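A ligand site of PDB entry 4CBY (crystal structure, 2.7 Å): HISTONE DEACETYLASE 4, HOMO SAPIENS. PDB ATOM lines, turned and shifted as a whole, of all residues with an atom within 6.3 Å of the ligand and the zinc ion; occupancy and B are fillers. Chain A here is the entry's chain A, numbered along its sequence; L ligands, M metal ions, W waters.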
ATOM      1  N   PRO A  32     -21.239   6.147 -30.200  1.00  0.00           N
ATOM      2  CA  PRO A  32     -20.421   6.206 -29.000  1.00  0.00           C
ATOM      3  C   PRO A  32     -19.144   5.404 -29.075  1.00  0.00           C
ATOM      4  O   PRO A  32     -18.136   5.814 -28.495  1.00  0.00           O
ATOM      5  CB  PRO A  32     -21.326   5.607 -27.923  1.00  0.00           C
ATOM      6  CG  PRO A  32     -22.719   5.721 -28.442  1.00  0.00           C
ATOM      7  CD  PRO A  32     -22.593   5.605 -29.928  1.00  0.00           C
ATOM      8  N   GLU A  33     -19.169   4.285 -29.778  1.00  0.00           N
ATOM      9  CA  GLU A  33     -17.989   3.455 -29.934  1.00  0.00           C
ATOM     10  C   GLU A  33     -17.184   3.981 -31.133  1.00  0.00           C
ATOM     11  O   GLU A  33     -17.230   3.453 -32.246  1.00  0.00           O
ATOM     12  CB  GLU A  33     -18.396   1.955 -29.993  1.00  0.00           C
ATOM     13  CG  GLU A  33     -17.659   0.978 -30.908  1.00  0.00           C
ATOM     14  CD  GLU A  33     -16.140   1.065 -30.909  1.00  0.00           C
ATOM     15  OE1 GLU A  33     -15.524   1.606 -29.970  1.00  0.00           O
ATOM     16  OE2 GLU A  33     -15.563   0.542 -31.892  1.00  0.00           O
ATOM     17  N   HIS A  34     -16.411   5.038 -30.877  1.00  0.00           N
ATOM     18  CA  HIS A  34     -15.715   5.755 -31.955  1.00  0.00           C
ATOM     19  C   HIS A  34     -14.214   5.638 -31.947  1.00  0.00           C
ATOM     20  O   HIS A  34     -13.611   5.376 -30.925  1.00  0.00           O
ATOM     21  CB  HIS A  34     -16.125   7.215 -31.949  1.00  0.00           C
ATOM     22  CG  HIS A  34     -15.753   7.951 -30.710  1.00  0.00           C
ATOM     23  ND1 HIS A  34     -14.668   8.759 -30.414  1.00  0.00           N
ATOM     24  CD2 HIS A  34     -16.525   7.928 -29.617  1.00  0.00           C
ATOM     25  CE1 HIS A  34     -14.824   9.198 -29.165  1.00  0.00           C
ATOM     26  NE2 HIS A  34     -15.949   8.671 -28.666  1.00  0.00           N
ATOM     27  N   ARG A  37     -11.536   6.812 -29.209  1.00  0.00           N
ATOM     28  CA  ARG A  37     -11.374   6.050 -27.965  1.00  0.00           C
ATOM     29  C   ARG A  37      -9.967   5.479 -27.831  1.00  0.00           C
ATOM     30  O   ARG A  37      -9.308   5.685 -26.814  1.00  0.00           O
ATOM     31  CB  ARG A  37     -12.420   4.947 -27.880  1.00  0.00           C
ATOM     32  CG  ARG A  37     -13.840   5.474 -27.710  1.00  0.00           C
ATOM     33  CD  ARG A  37     -14.862   4.429 -27.226  1.00  0.00           C
ATOM     34  NE  ARG A  37     -14.522   3.070 -27.635  1.00  0.00           N
ATOM     35  CZ  ARG A  37     -14.355   2.039 -26.808  1.00  0.00           C
ATOM     36  NH1 ARG A  37     -14.537   2.168 -25.504  1.00  0.00           N
ATOM     37  NH2 ARG A  37     -14.017   0.857 -27.304  1.00  0.00           N
ATOM     38  N   ASP A 115     -29.156  -0.618 -33.731  1.00  0.00           N
ATOM     39  CA  ASP A 115     -28.082   0.105 -33.061  1.00  0.00           C
ATOM     40  C   ASP A 115     -26.743   0.006 -33.787  1.00  0.00           C
ATOM     41  O   ASP A 115     -26.004   0.986 -33.875  1.00  0.00           O
ATOM     42  CB  ASP A 115     -27.922  -0.394 -31.615  1.00  0.00           C
ATOM     43  N   PRO A 156     -15.117  -3.579 -29.720  1.00  0.00           N
ATOM     44  CA  PRO A 156     -15.194  -4.496 -28.592  1.00  0.00           C
ATOM     45  C   PRO A 156     -15.785  -5.864 -28.948  1.00  0.00           C
ATOM     46  O   PRO A 156     -16.298  -6.050 -30.063  1.00  0.00           O
ATOM     47  CB  PRO A 156     -16.093  -3.750 -27.602  1.00  0.00           C
ATOM     48  CG  PRO A 156     -17.022  -2.978 -28.495  1.00  0.00           C
ATOM     49  CD  PRO A 156     -16.178  -2.559 -29.666  1.00  0.00           C
ATOM     50  N   HIS A 158     -17.193  -8.577 -26.179  1.00  0.00           N
ATOM     51  CA  HIS A 158     -17.850  -9.495 -25.243  1.00  0.00           C
ATOM     52  C   HIS A 158     -19.353  -9.706 -25.389  1.00  0.00           C
ATOM     53  O   HIS A 158     -19.940 -10.538 -24.683  1.00  0.00           O
ATOM     54  CB  HIS A 158     -17.432  -9.158 -23.810  1.00  0.00           C
ATOM     55  CG  HIS A 158     -18.061  -7.904 -23.243  1.00  0.00           C
ATOM     56  ND1 HIS A 158     -18.380  -7.789 -21.935  1.00  0.00           N
ATOM     57  CD2 HIS A 158     -18.433  -6.708 -23.840  1.00  0.00           C
ATOM     58  CE1 HIS A 158     -18.930  -6.581 -21.712  1.00  0.00           C
ATOM     59  NE2 HIS A 158     -18.960  -5.921 -22.879  1.00  0.00           N
ATOM     60  N   HIS A 159     -19.999  -8.982 -26.295  1.00  0.00           N
ATOM     61  CA  HIS A 159     -21.436  -9.168 -26.547  1.00  0.00           C
ATOM     62  C   HIS A 159     -21.700  -9.994 -27.768  1.00  0.00           C
ATOM     63  O   HIS A 159     -22.845 -10.392 -28.007  1.00  0.00           O
ATOM     64  CB  HIS A 159     -22.098  -7.817 -26.754  1.00  0.00           C
ATOM     65  CG  HIS A 159     -22.133  -6.968 -25.524  1.00  0.00           C
ATOM     66  ND1 HIS A 159     -22.785  -7.334 -24.420  1.00  0.00           N
ATOM     67  CD2 HIS A 159     -21.600  -5.719 -25.272  1.00  0.00           C
ATOM     68  CE1 HIS A 159     -22.671  -6.363 -23.485  1.00  0.00           C
ATOM     69  NE2 HIS A 159     -21.937  -5.370 -24.018  1.00  0.00           N
ATOM     70  N   GLY A 167     -24.424  -4.834 -29.380  1.00  0.00           N
ATOM     71  CA  GLY A 167     -23.668  -3.947 -28.490  1.00  0.00           C
ATOM     72  C   GLY A 167     -22.372  -3.449 -29.117  1.00  0.00           C
ATOM     73  O   GLY A 167     -21.357  -3.347 -28.449  1.00  0.00           O
ATOM     74  N   PHE A 168     -22.425  -3.189 -30.414  1.00  0.00           N
ATOM     75  CA  PHE A 168     -21.284  -2.699 -31.181  1.00  0.00           C
ATOM     76  C   PHE A 168     -20.134  -3.701 -31.275  1.00  0.00           C
ATOM     77  O   PHE A 168     -19.011  -3.340 -31.630  1.00  0.00           O
ATOM     78  CB  PHE A 168     -20.777  -1.347 -30.636  1.00  0.00           C
ATOM     79  CG  PHE A 168     -21.883  -0.336 -30.376  1.00  0.00           C
ATOM     80  CD1 PHE A 168     -22.997  -0.263 -31.194  1.00  0.00           C
ATOM     81  CD2 PHE A 168     -21.776   0.562 -29.332  1.00  0.00           C
ATOM     82  CE1 PHE A 168     -24.000   0.669 -30.950  1.00  0.00           C
ATOM     83  CE2 PHE A 168     -22.766   1.490 -29.086  1.00  0.00           C
ATOM     84  CZ  PHE A 168     -23.882   1.545 -29.890  1.00  0.00           C
ATOM     85  N   CYS A 169     -20.441  -4.970 -30.991  1.00  0.00           N
ATOM     86  CA  CYS A 169     -19.475  -6.055 -31.084  1.00  0.00           C
ATOM     87  C   CYS A 169     -19.800  -6.961 -32.260  1.00  0.00           C
ATOM     88  O   CYS A 169     -20.980  -7.210 -32.547  1.00  0.00           O
ATOM     89  CB  CYS A 169     -19.485  -6.873 -29.812  1.00  0.00           C
ATOM     90  SG  CYS A 169     -19.103  -5.944 -28.329  1.00  0.00           S
ATOM     91  N   ASP A 196     -15.994  -4.868 -17.181  1.00  0.00           N
ATOM     92  CA  ASP A 196     -16.844  -3.914 -17.895  1.00  0.00           C
ATOM     93  C   ASP A 196     -18.179  -3.865 -17.168  1.00  0.00           C
ATOM     94  O   ASP A 196     -18.656  -4.911 -16.692  1.00  0.00           O
ATOM     95  CB  ASP A 196     -17.052  -4.333 -19.355  1.00  0.00           C
ATOM     96  CG  ASP A 196     -17.920  -3.345 -20.157  1.00  0.00           C
ATOM     97  OD1 ASP A 196     -19.158  -3.322 -19.986  1.00  0.00           O
ATOM     98  OD2 ASP A 196     -17.364  -2.613 -20.999  1.00  0.00           O
ATOM     99  N   VAL A 197     -18.779  -2.687 -17.082  1.00  0.00           N
ATOM    100  CA  VAL A 197     -20.028  -2.511 -16.351  1.00  0.00           C
ATOM    101  C   VAL A 197     -21.178  -3.338 -16.943  1.00  0.00           C
ATOM    102  O   VAL A 197     -22.132  -3.635 -16.211  1.00  0.00           O
ATOM    103  CB  VAL A 197     -20.447  -1.026 -16.287  1.00  0.00           C
ATOM    104  CG1 VAL A 197     -20.989  -0.567 -17.638  1.00  0.00           C
ATOM    105  CG2 VAL A 197     -21.444  -0.785 -15.129  1.00  0.00           C
ATOM    106  N   HIS A 198     -21.093  -3.713 -18.219  1.00  0.00           N
ATOM    107  CA  HIS A 198     -22.124  -4.551 -18.856  1.00  0.00           C
ATOM    108  C   HIS A 198     -21.755  -6.014 -18.855  1.00  0.00           C
ATOM    109  O   HIS A 198     -20.563  -6.373 -18.922  1.00  0.00           O
ATOM    110  CB  HIS A 198     -22.380  -4.108 -20.309  1.00  0.00           C
ATOM    111  CG  HIS A 198     -22.758  -2.660 -20.438  1.00  0.00           C
ATOM    112  ND1 HIS A 198     -21.843  -1.705 -20.671  1.00  0.00           N
ATOM    113  CD2 HIS A 198     -23.984  -2.008 -20.367  1.00  0.00           C
ATOM    114  CE1 HIS A 198     -22.435  -0.512 -20.738  1.00  0.00           C
ATOM    115  NE2 HIS A 198     -23.752  -0.687 -20.541  1.00  0.00           N
ATOM    116  N   HIS A 199     -22.765  -6.883 -18.767  1.00  0.00           N
ATOM    117  CA  HIS A 199     -22.538  -8.334 -18.756  1.00  0.00           C
ATOM    118  C   HIS A 199     -22.008  -8.784 -20.070  1.00  0.00           C
ATOM    119  O   HIS A 199     -22.448  -8.301 -21.108  1.00  0.00           O
ATOM    120  CB  HIS A 199     -23.843  -9.071 -18.437  1.00  0.00           C
ATOM    121  CG  HIS A 199     -23.707 -10.585 -18.391  1.00  0.00           C
ATOM    122  ND1 HIS A 199     -24.388 -11.393 -19.225  1.00  0.00           N
ATOM    123  CD2 HIS A 199     -22.942 -11.421 -17.579  1.00  0.00           C
ATOM    124  CE1 HIS A 199     -24.061 -12.655 -18.967  1.00  0.00           C
ATOM    125  NE2 HIS A 199     -23.197 -12.677 -17.951  1.00  0.00           N
ATOM    126  N   PHE A 227     -28.811  -3.133 -19.878  1.00  0.00           N
ATOM    127  CA  PHE A 227     -28.276  -3.797 -21.064  1.00  0.00           C
ATOM    128  C   PHE A 227     -27.140  -4.733 -20.645  1.00  0.00           C
ATOM    129  O   PHE A 227     -26.328  -4.377 -19.792  1.00  0.00           O
ATOM    130  CB  PHE A 227     -27.786  -2.768 -22.079  1.00  0.00           C
ATOM    131  CG  PHE A 227     -27.260  -3.363 -23.330  1.00  0.00           C
ATOM    132  CD1 PHE A 227     -28.110  -3.749 -24.347  1.00  0.00           C
ATOM    133  CD2 PHE A 227     -25.893  -3.565 -23.493  1.00  0.00           C
ATOM    134  CE1 PHE A 227     -27.619  -4.332 -25.501  1.00  0.00           C
ATOM    135  CE2 PHE A 227     -25.383  -4.138 -24.646  1.00  0.00           C
ATOM    136  CZ  PHE A 227     -26.249  -4.505 -25.662  1.00  0.00           C
ATOM    137  N   GLY A 288     -13.323  -3.411 -19.640  1.00  0.00           N
ATOM    138  CA  GLY A 288     -14.124  -2.242 -19.980  1.00  0.00           C
ATOM    139  C   GLY A 288     -14.047  -1.242 -18.846  1.00  0.00           C
ATOM    140  O   GLY A 288     -13.983  -1.629 -17.680  1.00  0.00           O
ATOM    141  N   ASP A 290     -16.338   1.413 -18.429  1.00  0.00           N
ATOM    142  CA  ASP A 290     -17.590   2.182 -18.306  1.00  0.00           C
ATOM    143  C   ASP A 290     -18.158   2.249 -16.902  1.00  0.00           C
ATOM    144  O   ASP A 290     -19.131   2.971 -16.675  1.00  0.00           O
ATOM    145  CB  ASP A 290     -18.669   1.713 -19.290  1.00  0.00           C
ATOM    146  CG  ASP A 290     -18.650   0.238 -19.552  1.00  0.00           C
ATOM    147  OD1 ASP A 290     -18.035  -0.548 -18.785  1.00  0.00           O
ATOM    148  OD2 ASP A 290     -19.259  -0.124 -20.581  1.00  0.00           O
ATOM    149  N   PRO A 298     -27.860   5.569 -18.828  1.00  0.00           N
ATOM    150  CA  PRO A 298     -28.024   4.557 -19.877  1.00  0.00           C
ATOM    151  C   PRO A 298     -26.763   3.711 -20.096  1.00  0.00           C
ATOM    152  O   PRO A 298     -26.844   2.486 -20.196  1.00  0.00           O
ATOM    153  CB  PRO A 298     -28.326   5.392 -21.121  1.00  0.00           C
ATOM    154  CG  PRO A 298     -28.782   6.721 -20.596  1.00  0.00           C
ATOM    155  CD  PRO A 298     -27.999   6.932 -19.344  1.00  0.00           C
ATOM    156  N   LEU A 299     -25.615   4.373 -20.142  1.00  0.00           N
ATOM    157  CA  LEU A 299     -24.347   3.730 -20.494  1.00  0.00           C
ATOM    158  C   LEU A 299     -23.672   3.095 -19.279  1.00  0.00           C
ATOM    159  O   LEU A 299     -22.987   2.087 -19.396  1.00  0.00           O
ATOM    160  CB  LEU A 299     -23.429   4.769 -21.153  1.00  0.00           C
ATOM    161  CG  LEU A 299     -22.373   4.454 -22.234  1.00  0.00           C
ATOM    162  CD1 LEU A 299     -23.017   4.122 -23.589  1.00  0.00           C
ATOM    163  CD2 LEU A 299     -21.441   5.654 -22.380  1.00  0.00           C
ATOM    164  N   GLU A 329     -12.698  -3.387 -23.758  1.00  0.00           N
ATOM    165  CA  GLU A 329     -14.067  -3.624 -24.170  1.00  0.00           C
ATOM    166  C   GLU A 329     -14.755  -2.250 -24.213  1.00  0.00           C
ATOM    167  O   GLU A 329     -14.407  -1.433 -25.081  1.00  0.00           O
ATOM    168  CB  GLU A 329     -14.773  -4.610 -23.237  1.00  0.00           C
ATOM    169  CG  GLU A 329     -14.181  -6.023 -23.216  1.00  0.00           C
ATOM    170  CD  GLU A 329     -14.538  -6.887 -24.420  1.00  0.00           C
ATOM    171  OE1 GLU A 329     -15.280  -6.428 -25.309  1.00  0.00           O
ATOM    172  OE2 GLU A 329     -14.051  -8.033 -24.491  1.00  0.00           O
ATOM    173  N   GLY A 330     -15.671  -1.959 -23.285  1.00  0.00           N
ATOM    174  CA  GLY A 330     -16.374  -0.668 -23.247  1.00  0.00           C
ATOM    175  C   GLY A 330     -15.605   0.454 -22.543  1.00  0.00           C
ATOM    176  O   GLY A 330     -14.422   0.307 -22.214  1.00  0.00           O
ATOM    177  N   GLY A 331     -16.304   1.583 -22.341  1.00  0.00           N
ATOM    178  CA  GLY A 331     -15.713   2.786 -21.767  1.00  0.00           C
ATOM    179  C   GLY A 331     -15.650   3.926 -22.761  1.00  0.00           C
ATOM    180  O   GLY A 331     -14.942   3.823 -23.759  1.00  0.00           O
ATOM    181  N   HIS A 332     -16.393   5.006 -22.501  1.00  0.00           N
ATOM    182  CA  HIS A 332     -16.668   6.066 -23.490  1.00  0.00           C
ATOM    183  C   HIS A 332     -15.964   7.343 -23.194  1.00  0.00           C
ATOM    184  O   HIS A 332     -15.294   7.925 -24.048  1.00  0.00           O
ATOM    185  CB  HIS A 332     -18.180   6.308 -23.557  1.00  0.00           C
ATOM    186  CG  HIS A 332     -18.578   7.491 -24.396  1.00  0.00           C
ATOM    187  ND1 HIS A 332     -18.906   7.385 -25.702  1.00  0.00           N
ATOM    188  CD2 HIS A 332     -18.745   8.828 -24.070  1.00  0.00           C
ATOM    189  CE1 HIS A 332     -19.240   8.596 -26.176  1.00  0.00           C
ATOM    190  NE2 HIS A 332     -19.134   9.474 -25.179  1.00  0.00           N
HETATM  191  C1  LIG L   1     -20.820  -1.534 -23.627  1.00  0.00           C
HETATM  192  C2  LIG L   1     -21.891  -1.222 -24.665  1.00  0.00           C
HETATM  193  C3  LIG L   1     -22.603   0.144 -24.813  1.00  0.00           C
HETATM  194  C4  LIG L   1     -21.545  -0.299 -25.832  1.00  0.00           C
HETATM  195  C5  LIG L   1     -24.061  -0.005 -25.129  1.00  0.00           C
HETATM  196  C6  LIG L   1     -24.930   0.213 -24.060  1.00  0.00           C
HETATM  197  C7  LIG L   1     -26.295   0.103 -24.202  1.00  0.00           C
HETATM  198  C8  LIG L   1     -26.842  -0.224 -25.433  1.00  0.00           C
HETATM  199  C9  LIG L   1     -25.995  -0.465 -26.519  1.00  0.00           C
HETATM  200  C10 LIG L   1     -24.597  -0.349 -26.374  1.00  0.00           C
HETATM  201  C11 LIG L   1     -20.356   0.577 -25.873  1.00  0.00           C
HETATM  202  C12 LIG L   1     -19.092   0.017 -26.048  1.00  0.00           C
HETATM  203  C13 LIG L   1     -17.982   0.847 -26.132  1.00  0.00           C
HETATM  204  C14 LIG L   1     -18.118   2.236 -26.055  1.00  0.00           C
HETATM  205  C15 LIG L   1     -19.392   2.792 -25.914  1.00  0.00           C
HETATM  206  C16 LIG L   1     -20.502   1.962 -25.830  1.00  0.00           C
HETATM  207  C17 LIG L   1     -28.322  -0.341 -25.502  1.00  0.00           C
HETATM  208  O1  LIG L   1     -29.036  -1.303 -26.173  1.00  0.00           O
HETATM  209  C18 LIG L   1     -30.387  -1.073 -25.945  1.00  0.00           C
HETATM  210  N1  LIG L   1     -30.491   0.014 -25.136  1.00  0.00           N
HETATM  211  C19 LIG L   1     -29.247   0.475 -24.845  1.00  0.00           C
HETATM  212  O2  LIG L   1     -20.322  -0.754 -22.810  1.00  0.00           O
HETATM  213  N2  LIG L   1     -20.514  -2.826 -23.675  1.00  0.00           N
HETATM  214  O3  LIG L   1     -19.639  -3.428 -22.767  1.00  0.00           O
HETATM  215 ZN    ZN M   1     -19.808  -1.881 -21.250  1.00  0.00          ZN
HETATM  216  O   HOH W   1     -19.522   2.082 -22.294  1.00  0.00           O
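A ring nitrogen (NE2) of His 158 lies close to an oxygen (O3) of the ligand (2.6 Å).
N2 of the ligand sits at hydrogen-bond distance from NE2 of His 159, 2.9 Å away.
N of Val 197 is in hydrogen-bond range of OD1 of Asp 290, 2.8 Å away.
The side-chain carboxylate of Asp 196 lies close to the backbone NH of Gly 330.
A ring nitrogen (NE2) of His 198 sits close to the backbone carbonyl oxygen (O) of Leu 299 (3.1 Å).
A ring nitrogen (NE2) of His 158 lies within hydrogen-bond range of a ring nitrogen (NE2) of His 159 (3.2 Å).
The backbone NH of His 159 lies within hydrogen-bond range of the side-chain sulfur of Cys 169 (3.8 Å).
NE of Arg 37 is in salt-bridge range of OE1 of Glu 33.
NH2 of Arg 37 is in hydrogen-bond range of O of Glu 329.
The backbone carbonyl oxygen of Pro 32 sits at hydrogen-bond distance from a ring nitrogen (ND1) of His 332 (3.3 Å).
Merely in contact with the ligand: Phe 227 (3.2 Å), Phe 168 (3.6 Å), Arg 37 (3.6 Å), Gly 330 (3.6 Å), Glu 33 (3.96 Å) and Pro 32 (3.96 Å).
Within 4 Å of the zinc ion: Asp 196, His 198 and Asp 290.
The nearest printed residue that does not touch the zinc ion is Val 197 (4.02 Å).
The zinc ion is bound by OD2 of Asp 290 (2.0 Å).
O2 of the ligand is bound to the zinc ion.
The side-chain carboxylate (OD1) of Asp 196 binds the zinc ion (2.0 Å).
The zinc ion is bound by ND1 of His 198.
The zinc ion is bound by an oxygen (O3) of the ligand (2.2 Å).
OD2 of Asp 196 binds the zinc ion (2.6 Å).
The zinc ion has six donor atoms within binding distance.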
